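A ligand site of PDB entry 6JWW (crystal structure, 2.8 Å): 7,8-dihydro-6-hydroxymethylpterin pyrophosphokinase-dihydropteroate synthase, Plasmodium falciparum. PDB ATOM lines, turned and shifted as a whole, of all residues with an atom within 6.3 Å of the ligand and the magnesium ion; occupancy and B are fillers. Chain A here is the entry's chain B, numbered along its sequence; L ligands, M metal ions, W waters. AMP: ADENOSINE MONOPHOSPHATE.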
ATOM      1  N   LEU A 181     -12.692  18.943   0.822  1.00  0.00           N
ATOM      2  CA  LEU A 181     -11.627  19.505   1.664  1.00  0.00           C
ATOM      3  C   LEU A 181     -11.166  20.888   1.184  1.00  0.00           C
ATOM      4  O   LEU A 181     -10.870  21.756   2.006  1.00  0.00           O
ATOM      5  CB  LEU A 181     -10.442  18.527   1.776  1.00  0.00           C
ATOM      6  CG  LEU A 181      -9.276  18.844   2.732  1.00  0.00           C
ATOM      7  CD1 LEU A 181      -9.738  19.169   4.137  1.00  0.00           C
ATOM      8  CD2 LEU A 181      -8.295  17.684   2.746  1.00  0.00           C
ATOM      9  N   ILE A 184     -14.244  22.920   2.296  1.00  0.00           N
ATOM     10  CA  ILE A 184     -14.156  22.944   3.764  1.00  0.00           C
ATOM     11  C   ILE A 184     -13.115  23.966   4.254  1.00  0.00           C
ATOM     12  O   ILE A 184     -13.411  24.778   5.149  1.00  0.00           O
ATOM     13  CB  ILE A 184     -13.920  21.526   4.352  1.00  0.00           C
ATOM     14  CG1 ILE A 184     -15.273  20.842   4.537  1.00  0.00           C
ATOM     15  CG2 ILE A 184     -13.132  21.557   5.673  1.00  0.00           C
ATOM     16  CD1 ILE A 184     -15.217  19.415   5.028  1.00  0.00           C
ATOM     17  N   LYS A 185     -11.922  23.930   3.668  1.00  0.00           N
ATOM     18  CA  LYS A 185     -10.849  24.826   4.086  1.00  0.00           C
ATOM     19  C   LYS A 185     -11.088  26.269   3.630  1.00  0.00           C
ATOM     20  O   LYS A 185     -10.641  27.195   4.289  1.00  0.00           O
ATOM     21  CB  LYS A 185      -9.460  24.301   3.669  1.00  0.00           C
ATOM     22  CG  LYS A 185      -9.027  22.993   4.338  1.00  0.00           C
ATOM     23  CD  LYS A 185      -8.658  23.125   5.808  1.00  0.00           C
ATOM     24  CE  LYS A 185      -8.776  21.795   6.539  1.00  0.00           C
ATOM     25  NZ  LYS A 185      -8.983  21.933   8.005  1.00  0.00           N
ATOM     26  N   GLU A 188     -13.473  27.441   6.305  1.00  0.00           N
ATOM     27  CA  GLU A 188     -12.579  27.804   7.420  1.00  0.00           C
ATOM     28  C   GLU A 188     -11.931  29.162   7.237  1.00  0.00           C
ATOM     29  O   GLU A 188     -11.953  29.996   8.138  1.00  0.00           O
ATOM     30  CB  GLU A 188     -11.492  26.743   7.594  1.00  0.00           C
ATOM     31  CG  GLU A 188     -11.717  25.772   8.742  1.00  0.00           C
ATOM     32  CD  GLU A 188     -10.936  24.486   8.565  1.00  0.00           C
ATOM     33  OE1 GLU A 188      -9.990  24.241   9.343  1.00  0.00           O
ATOM     34  OE2 GLU A 188     -11.270  23.719   7.639  1.00  0.00           O
ATOM     35  N   ASP A 208     -12.082  24.383  13.357  1.00  0.00           N
ATOM     36  CA  ASP A 208     -11.489  23.286  12.634  1.00  0.00           C
ATOM     37  C   ASP A 208     -12.599  22.327  12.182  1.00  0.00           C
ATOM     38  O   ASP A 208     -13.373  21.821  13.004  1.00  0.00           O
ATOM     39  CB  ASP A 208     -10.468  22.571  13.518  1.00  0.00           C
ATOM     40  CG  ASP A 208      -9.531  21.655  12.744  1.00  0.00           C
ATOM     41  OD1 ASP A 208      -9.067  22.035  11.637  1.00  0.00           O
ATOM     42  OD2 ASP A 208      -9.246  20.544  13.236  1.00  0.00           O
ATOM     43  N   ILE A 209     -12.675  22.110  10.868  1.00  0.00           N
ATOM     44  CA  ILE A 209     -13.621  21.191  10.247  1.00  0.00           C
ATOM     45  C   ILE A 209     -12.830  20.088   9.550  1.00  0.00           C
ATOM     46  O   ILE A 209     -12.052  20.365   8.638  1.00  0.00           O
ATOM     47  CB  ILE A 209     -14.570  21.889   9.236  1.00  0.00           C
ATOM     48  CG1 ILE A 209     -15.171  23.183   9.813  1.00  0.00           C
ATOM     49  CG2 ILE A 209     -15.676  20.948   8.772  1.00  0.00           C
ATOM     50  CD1 ILE A 209     -15.747  24.132   8.784  1.00  0.00           C
ATOM     51  N   ASP A 210     -13.012  18.857  10.007  1.00  0.00           N
ATOM     52  CA  ASP A 210     -12.372  17.673   9.412  1.00  0.00           C
ATOM     53  C   ASP A 210     -13.405  16.883   8.616  1.00  0.00           C
ATOM     54  O   ASP A 210     -14.602  17.177   8.681  1.00  0.00           O
ATOM     55  CB  ASP A 210     -11.753  16.783  10.512  1.00  0.00           C
ATOM     56  CG  ASP A 210     -10.623  17.483  11.286  1.00  0.00           C
ATOM     57  OD1 ASP A 210      -9.439  17.406  10.860  1.00  0.00           O
ATOM     58  OD2 ASP A 210     -10.922  18.086  12.338  1.00  0.00           O
ATOM     59  N   ILE A 211     -12.942  15.877   7.866  1.00  0.00           N
ATOM     60  CA  ILE A 211     -13.834  14.967   7.147  1.00  0.00           C
ATOM     61  C   ILE A 211     -13.616  13.553   7.667  1.00  0.00           C
ATOM     62  O   ILE A 211     -12.601  12.911   7.361  1.00  0.00           O
ATOM     63  CB  ILE A 211     -13.603  15.012   5.604  1.00  0.00           C
ATOM     64  CG1 ILE A 211     -13.724  16.452   5.081  1.00  0.00           C
ATOM     65  CG2 ILE A 211     -14.569  14.059   4.889  1.00  0.00           C
ATOM     66  CD1 ILE A 211     -13.117  16.692   3.710  1.00  0.00           C
ATOM     67  N   LEU A 212     -14.569  13.077   8.455  1.00  0.00           N
ATOM     68  CA  LEU A 212     -14.456  11.769   9.099  1.00  0.00           C
ATOM     69  C   LEU A 212     -14.720  10.596   8.185  1.00  0.00           C
ATOM     70  O   LEU A 212     -14.091   9.554   8.325  1.00  0.00           O
ATOM     71  CB  LEU A 212     -15.358  11.692  10.343  1.00  0.00           C
ATOM     72  CG  LEU A 212     -15.205  12.803  11.383  1.00  0.00           C
ATOM     73  CD1 LEU A 212     -16.204  12.610  12.511  1.00  0.00           C
ATOM     74  CD2 LEU A 212     -13.780  12.888  11.925  1.00  0.00           C
ATOM     75  N   ASN A 312      -1.772  24.234   3.637  1.00  0.00           N
ATOM     76  CA  ASN A 312      -2.486  23.385   4.585  1.00  0.00           C
ATOM     77  C   ASN A 312      -2.883  22.006   4.045  1.00  0.00           C
ATOM     78  O   ASN A 312      -2.911  21.046   4.810  1.00  0.00           O
ATOM     79  CB  ASN A 312      -3.700  24.116   5.206  1.00  0.00           C
ATOM     80  CG  ASN A 312      -3.377  24.740   6.569  1.00  0.00           C
ATOM     81  OD1 ASN A 312      -2.217  24.970   6.923  1.00  0.00           O
ATOM     82  ND2 ASN A 312      -4.433  25.028   7.335  1.00  0.00           N
ATOM     83  N   ILE A 313      -3.157  21.913   2.747  1.00  0.00           N
ATOM     84  CA  ILE A 313      -3.531  20.621   2.147  1.00  0.00           C
ATOM     85  C   ILE A 313      -2.276  19.782   1.839  1.00  0.00           C
ATOM     86  O   ILE A 313      -1.875  19.613   0.671  1.00  0.00           O
ATOM     87  CB  ILE A 313      -4.467  20.751   0.911  1.00  0.00           C
ATOM     88  CG1 ILE A 313      -5.353  22.012   1.032  1.00  0.00           C
ATOM     89  CG2 ILE A 313      -5.246  19.445   0.702  1.00  0.00           C
ATOM     90  CD1 ILE A 313      -6.737  21.946   0.319  1.00  0.00           C
ATOM     91  N   GLU A 314      -1.668  19.275   2.906  1.00  0.00           N
ATOM     92  CA  GLU A 314      -0.466  18.456   2.801  1.00  0.00           C
ATOM     93  C   GLU A 314      -0.822  17.008   2.490  1.00  0.00           C
ATOM     94  O   GLU A 314      -0.118  16.347   1.718  1.00  0.00           O
ATOM     95  CB  GLU A 314       0.396  18.541   4.076  1.00  0.00           C
ATOM     96  CG  GLU A 314       0.571  19.964   4.627  1.00  0.00           C
ATOM     97  CD  GLU A 314       2.004  20.340   4.963  1.00  0.00           C
ATOM     98  OE1 GLU A 314       2.205  21.179   5.874  1.00  0.00           O
ATOM     99  OE2 GLU A 314       2.954  19.822   4.320  1.00  0.00           O
ATOM    100  N   PHE A 315      -1.921  16.521   3.072  1.00  0.00           N
ATOM    101  CA  PHE A 315      -2.400  15.138   2.856  1.00  0.00           C
ATOM    102  C   PHE A 315      -3.920  14.956   3.095  1.00  0.00           C
ATOM    103  O   PHE A 315      -4.622  15.912   3.467  1.00  0.00           O
ATOM    104  CB  PHE A 315      -1.538  14.137   3.661  1.00  0.00           C
ATOM    105  CG  PHE A 315      -1.943  13.978   5.104  1.00  0.00           C
ATOM    106  CD1 PHE A 315      -1.797  15.022   6.027  1.00  0.00           C
ATOM    107  CD2 PHE A 315      -2.438  12.757   5.552  1.00  0.00           C
ATOM    108  CE1 PHE A 315      -2.163  14.851   7.353  1.00  0.00           C
ATOM    109  CE2 PHE A 315      -2.810  12.580   6.883  1.00  0.00           C
ATOM    110  CZ  PHE A 315      -2.672  13.627   7.784  1.00  0.00           C
ATOM    111  N   LEU A 316      -4.419  13.738   2.864  1.00  0.00           N
ATOM    112  CA  LEU A 316      -5.838  13.385   3.031  1.00  0.00           C
ATOM    113  C   LEU A 316      -6.055  11.932   3.458  1.00  0.00           C
ATOM    114  O   LEU A 316      -5.669  10.995   2.745  1.00  0.00           O
ATOM    115  CB  LEU A 316      -6.633  13.670   1.749  1.00  0.00           C
ATOM    116  CG  LEU A 316      -8.038  13.060   1.572  1.00  0.00           C
ATOM    117  CD1 LEU A 316      -9.095  13.710   2.471  1.00  0.00           C
ATOM    118  CD2 LEU A 316      -8.465  13.110   0.105  1.00  0.00           C
ATOM    119  N   SER A 317      -6.704  11.760   4.612  1.00  0.00           N
ATOM    120  CA  SER A 317      -7.074  10.428   5.113  1.00  0.00           C
ATOM    121  C   SER A 317      -8.588  10.227   5.264  1.00  0.00           C
ATOM    122  O   SER A 317      -9.253  10.965   6.002  1.00  0.00           O
ATOM    123  CB  SER A 317      -6.358  10.114   6.428  1.00  0.00           C
ATOM    124  OG  SER A 317      -6.477   8.738   6.750  1.00  0.00           O
ATOM    125  N   ILE A 318      -9.117   9.227   4.569  1.00  0.00           N
ATOM    126  CA  ILE A 318     -10.529   8.843   4.653  1.00  0.00           C
ATOM    127  C   ILE A 318     -10.590   7.334   4.993  1.00  0.00           C
ATOM    128  O   ILE A 318     -10.109   6.523   4.209  1.00  0.00           O
ATOM    129  CB  ILE A 318     -11.320   9.160   3.340  1.00  0.00           C
ATOM    130  CG1 ILE A 318     -11.331  10.677   3.010  1.00  0.00           C
ATOM    131  CG2 ILE A 318     -12.734   8.577   3.381  1.00  0.00           C
ATOM    132  CD1 ILE A 318     -12.013  11.596   4.002  1.00  0.00           C
ATOM    133  N   PRO A 319     -11.133   6.959   6.151  1.00  0.00           N
ATOM    134  CA  PRO A 319     -11.597   7.866   7.200  1.00  0.00           C
ATOM    135  C   PRO A 319     -10.459   8.644   7.854  1.00  0.00           C
ATOM    136  O   PRO A 319      -9.296   8.323   7.637  1.00  0.00           O
ATOM    137  CB  PRO A 319     -12.252   6.923   8.228  1.00  0.00           C
ATOM    138  CG  PRO A 319     -11.744   5.557   7.908  1.00  0.00           C
ATOM    139  CD  PRO A 319     -11.494   5.552   6.436  1.00  0.00           C
ATOM    140  N   HIS A 320     -10.810   9.664   8.639  1.00  0.00           N
ATOM    141  CA  HIS A 320      -9.849  10.486   9.383  1.00  0.00           C
ATOM    142  C   HIS A 320      -8.933   9.621  10.248  1.00  0.00           C
ATOM    143  O   HIS A 320      -9.295   8.495  10.628  1.00  0.00           O
ATOM    144  CB  HIS A 320     -10.594  11.490  10.265  1.00  0.00           C
ATOM    145  CG  HIS A 320      -9.805  12.711  10.603  1.00  0.00           C
ATOM    146  ND1 HIS A 320      -8.971  12.777  11.706  1.00  0.00           N
ATOM    147  CD2 HIS A 320      -9.740  13.928  10.017  1.00  0.00           C
ATOM    148  CE1 HIS A 320      -8.428  13.983  11.770  1.00  0.00           C
ATOM    149  NE2 HIS A 320      -8.878  14.691  10.759  1.00  0.00           N
ATOM    150  N   VAL A 321      -7.744  10.136  10.536  1.00  0.00           N
ATOM    151  CA  VAL A 321      -6.723   9.423  11.298  1.00  0.00           C
ATOM    152  C   VAL A 321      -7.233   9.099  12.705  1.00  0.00           C
ATOM    153  O   VAL A 321      -7.306   7.932  13.109  1.00  0.00           O
ATOM    154  CB  VAL A 321      -5.394  10.197  11.349  1.00  0.00           C
ATOM    155  CG1 VAL A 321      -4.318   9.404  12.076  1.00  0.00           C
ATOM    156  CG2 VAL A 321      -4.902  10.533   9.955  1.00  0.00           C
ATOM    157  N   ARG A 326      -9.428   9.354  19.008  1.00  0.00           N
ATOM    158  CA  ARG A 326      -9.990  10.447  19.794  1.00  0.00           C
ATOM    159  C   ARG A 326     -11.375  10.063  20.316  1.00  0.00           C
ATOM    160  O   ARG A 326     -12.300   9.808  19.538  1.00  0.00           O
ATOM    161  CB  ARG A 326     -10.069  11.749  18.982  1.00  0.00           C
ATOM    162  CG  ARG A 326      -8.775  12.547  18.900  1.00  0.00           C
ATOM    163  CD  ARG A 326      -9.035  13.935  18.326  1.00  0.00           C
ATOM    164  NE  ARG A 326      -7.974  14.390  17.425  1.00  0.00           N
ATOM    165  CZ  ARG A 326      -8.138  15.296  16.448  1.00  0.00           C
ATOM    166  NH1 ARG A 326      -9.332  15.851  16.216  1.00  0.00           N
ATOM    167  NH2 ARG A 326      -7.108  15.631  15.686  1.00  0.00           N
HETATM  168  P   AMP L   1      -5.664  19.941  11.881  1.00  0.00           P
HETATM  169  O1P AMP L   1      -5.629  21.445  12.099  1.00  0.00           O
HETATM  170  O2P AMP L   1      -4.736  19.159  12.778  1.00  0.00           O
HETATM  171  O3P AMP L   1      -7.062  19.379  11.783  1.00  0.00           O
HETATM  172  O5' AMP L   1      -5.013  19.748  10.413  1.00  0.00           O
HETATM  173  C5' AMP L   1      -5.143  18.536   9.676  1.00  0.00           C
HETATM  174  C4' AMP L   1      -4.692  18.769   8.235  1.00  0.00           C
HETATM  175  O4' AMP L   1      -4.395  17.523   7.611  1.00  0.00           O
HETATM  176  C3' AMP L   1      -5.768  19.436   7.386  1.00  0.00           C
HETATM  177  O3' AMP L   1      -5.534  20.847   7.267  1.00  0.00           O
HETATM  178  C2' AMP L   1      -5.728  18.722   6.047  1.00  0.00           C
HETATM  179  O2' AMP L   1      -4.974  19.424   5.046  1.00  0.00           O
HETATM  180  C1' AMP L   1      -5.049  17.392   6.345  1.00  0.00           C
HETATM  181  N9  AMP L   1      -5.992  16.229   6.383  1.00  0.00           N
HETATM  182  C8  AMP L   1      -5.598  14.960   6.220  1.00  0.00           C
HETATM  183  N7  AMP L   1      -6.630  14.087   6.296  1.00  0.00           N
HETATM  184  C5  AMP L   1      -7.749  14.797   6.505  1.00  0.00           C
HETATM  185  C6  AMP L   1      -9.195  14.509   6.681  1.00  0.00           C
HETATM  186  N6  AMP L   1      -9.680  13.249   6.650  1.00  0.00           N
HETATM  187  N1  AMP L   1     -10.039  15.543   6.892  1.00  0.00           N
HETATM  188  C2  AMP L   1      -9.591  16.807   6.946  1.00  0.00           C
HETATM  189  N3  AMP L   1      -8.298  17.147   6.786  1.00  0.00           N
HETATM  190  C4  AMP L   1      -7.334  16.213   6.570  1.00  0.00           C
HETATM  191 MG    MG M   1      -8.447  19.896  10.555  1.00  0.00          MG
HETATM  192  O   HOH W   1      -5.326  22.516   9.301  1.00  0.00           O
HETATM  193  O   HOH W   2      -8.506  17.426  13.720  1.00  0.00           O
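The side-chain hydroxyl (OG) of Ser 317 sits at hydrogen-bond distance from the backbone carbonyl oxygen (O) of Pro 319. The side-chain carboxylate of Asp 208 sits close to the side-chain amino group of Lys 185 (3.6 Å). OD1 of Asp 210 is in hydrogen-bond range of NE2 of His 320. The side-chain amino group of Lys 185 lies within salt-bridge range of the side-chain carboxylate of Glu 188. N of His 320 lies within hydrogen-bond range of O of Leu 212.
The backbone NH of Ser 317 lies within hydrogen-bond range of a nitrogen (N7) of the ligand. The backbone carbonyl oxygen (O) of Ser 317 lies within hydrogen-bond range of a nitrogen (N6) of the ligand (2.4 Å). The backbone carbonyl oxygen (O) of Asn 312 sits at hydrogen-bond distance from an oxygen (O2') of the ligand (2.6 Å). N1 of the ligand sits at hydrogen-bond distance from N of Ile 211 (3.1 Å). A nitrogen (N6) of the ligand sits at hydrogen-bond distance from the backbone carbonyl oxygen (O) of Ile 211, at 3.0 Å.
Water W1 bridges O3' of the ligand (2.6 Å) and ND2 of Asn 312 (3.3 Å). Water W2 lies within hydrogen-bond range of the side-chain carboxylate (OD2) of Asp 210, the guanidinium group (NH2) of Arg 326 and the side-chain carboxylate (OD2) of Asp 208.
Residues that only touch the magnesium ion: Lys 185 (3.3 Å). Of the 20 residues printed, 3 come within 4 Å of the magnesium ion. The nearest printed residue that does not touch the magnesium ion is Ile 209 (4.1 Å).
The magnesium ion is bound by an oxygen (O3P) of the ligand (1.9 Å) and the side-chain carboxylate (OD1) of Asp 208 (2.5 Å). Slightly farther from the magnesium ion lies the side-chain carboxylate (OD1) of Asp 210 (2.7 Å).
The backbone carbonyl oxygen (O) of Phe 315 lies close to a nitrogen (N9) of the ligand (3.2 Å). Residues that only touch the ligand: Leu 181, Lys 185, Ile 313, Glu 314, Leu 316, Ile 318 and His 320. Hydrophobic or aromatic side chains within 4 Å of the ligand: Leu 181, Ile 211, Phe 315, Ile 318 and His 320. Of the 20 residues printed, 13 come within 4 Å of the ligand.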
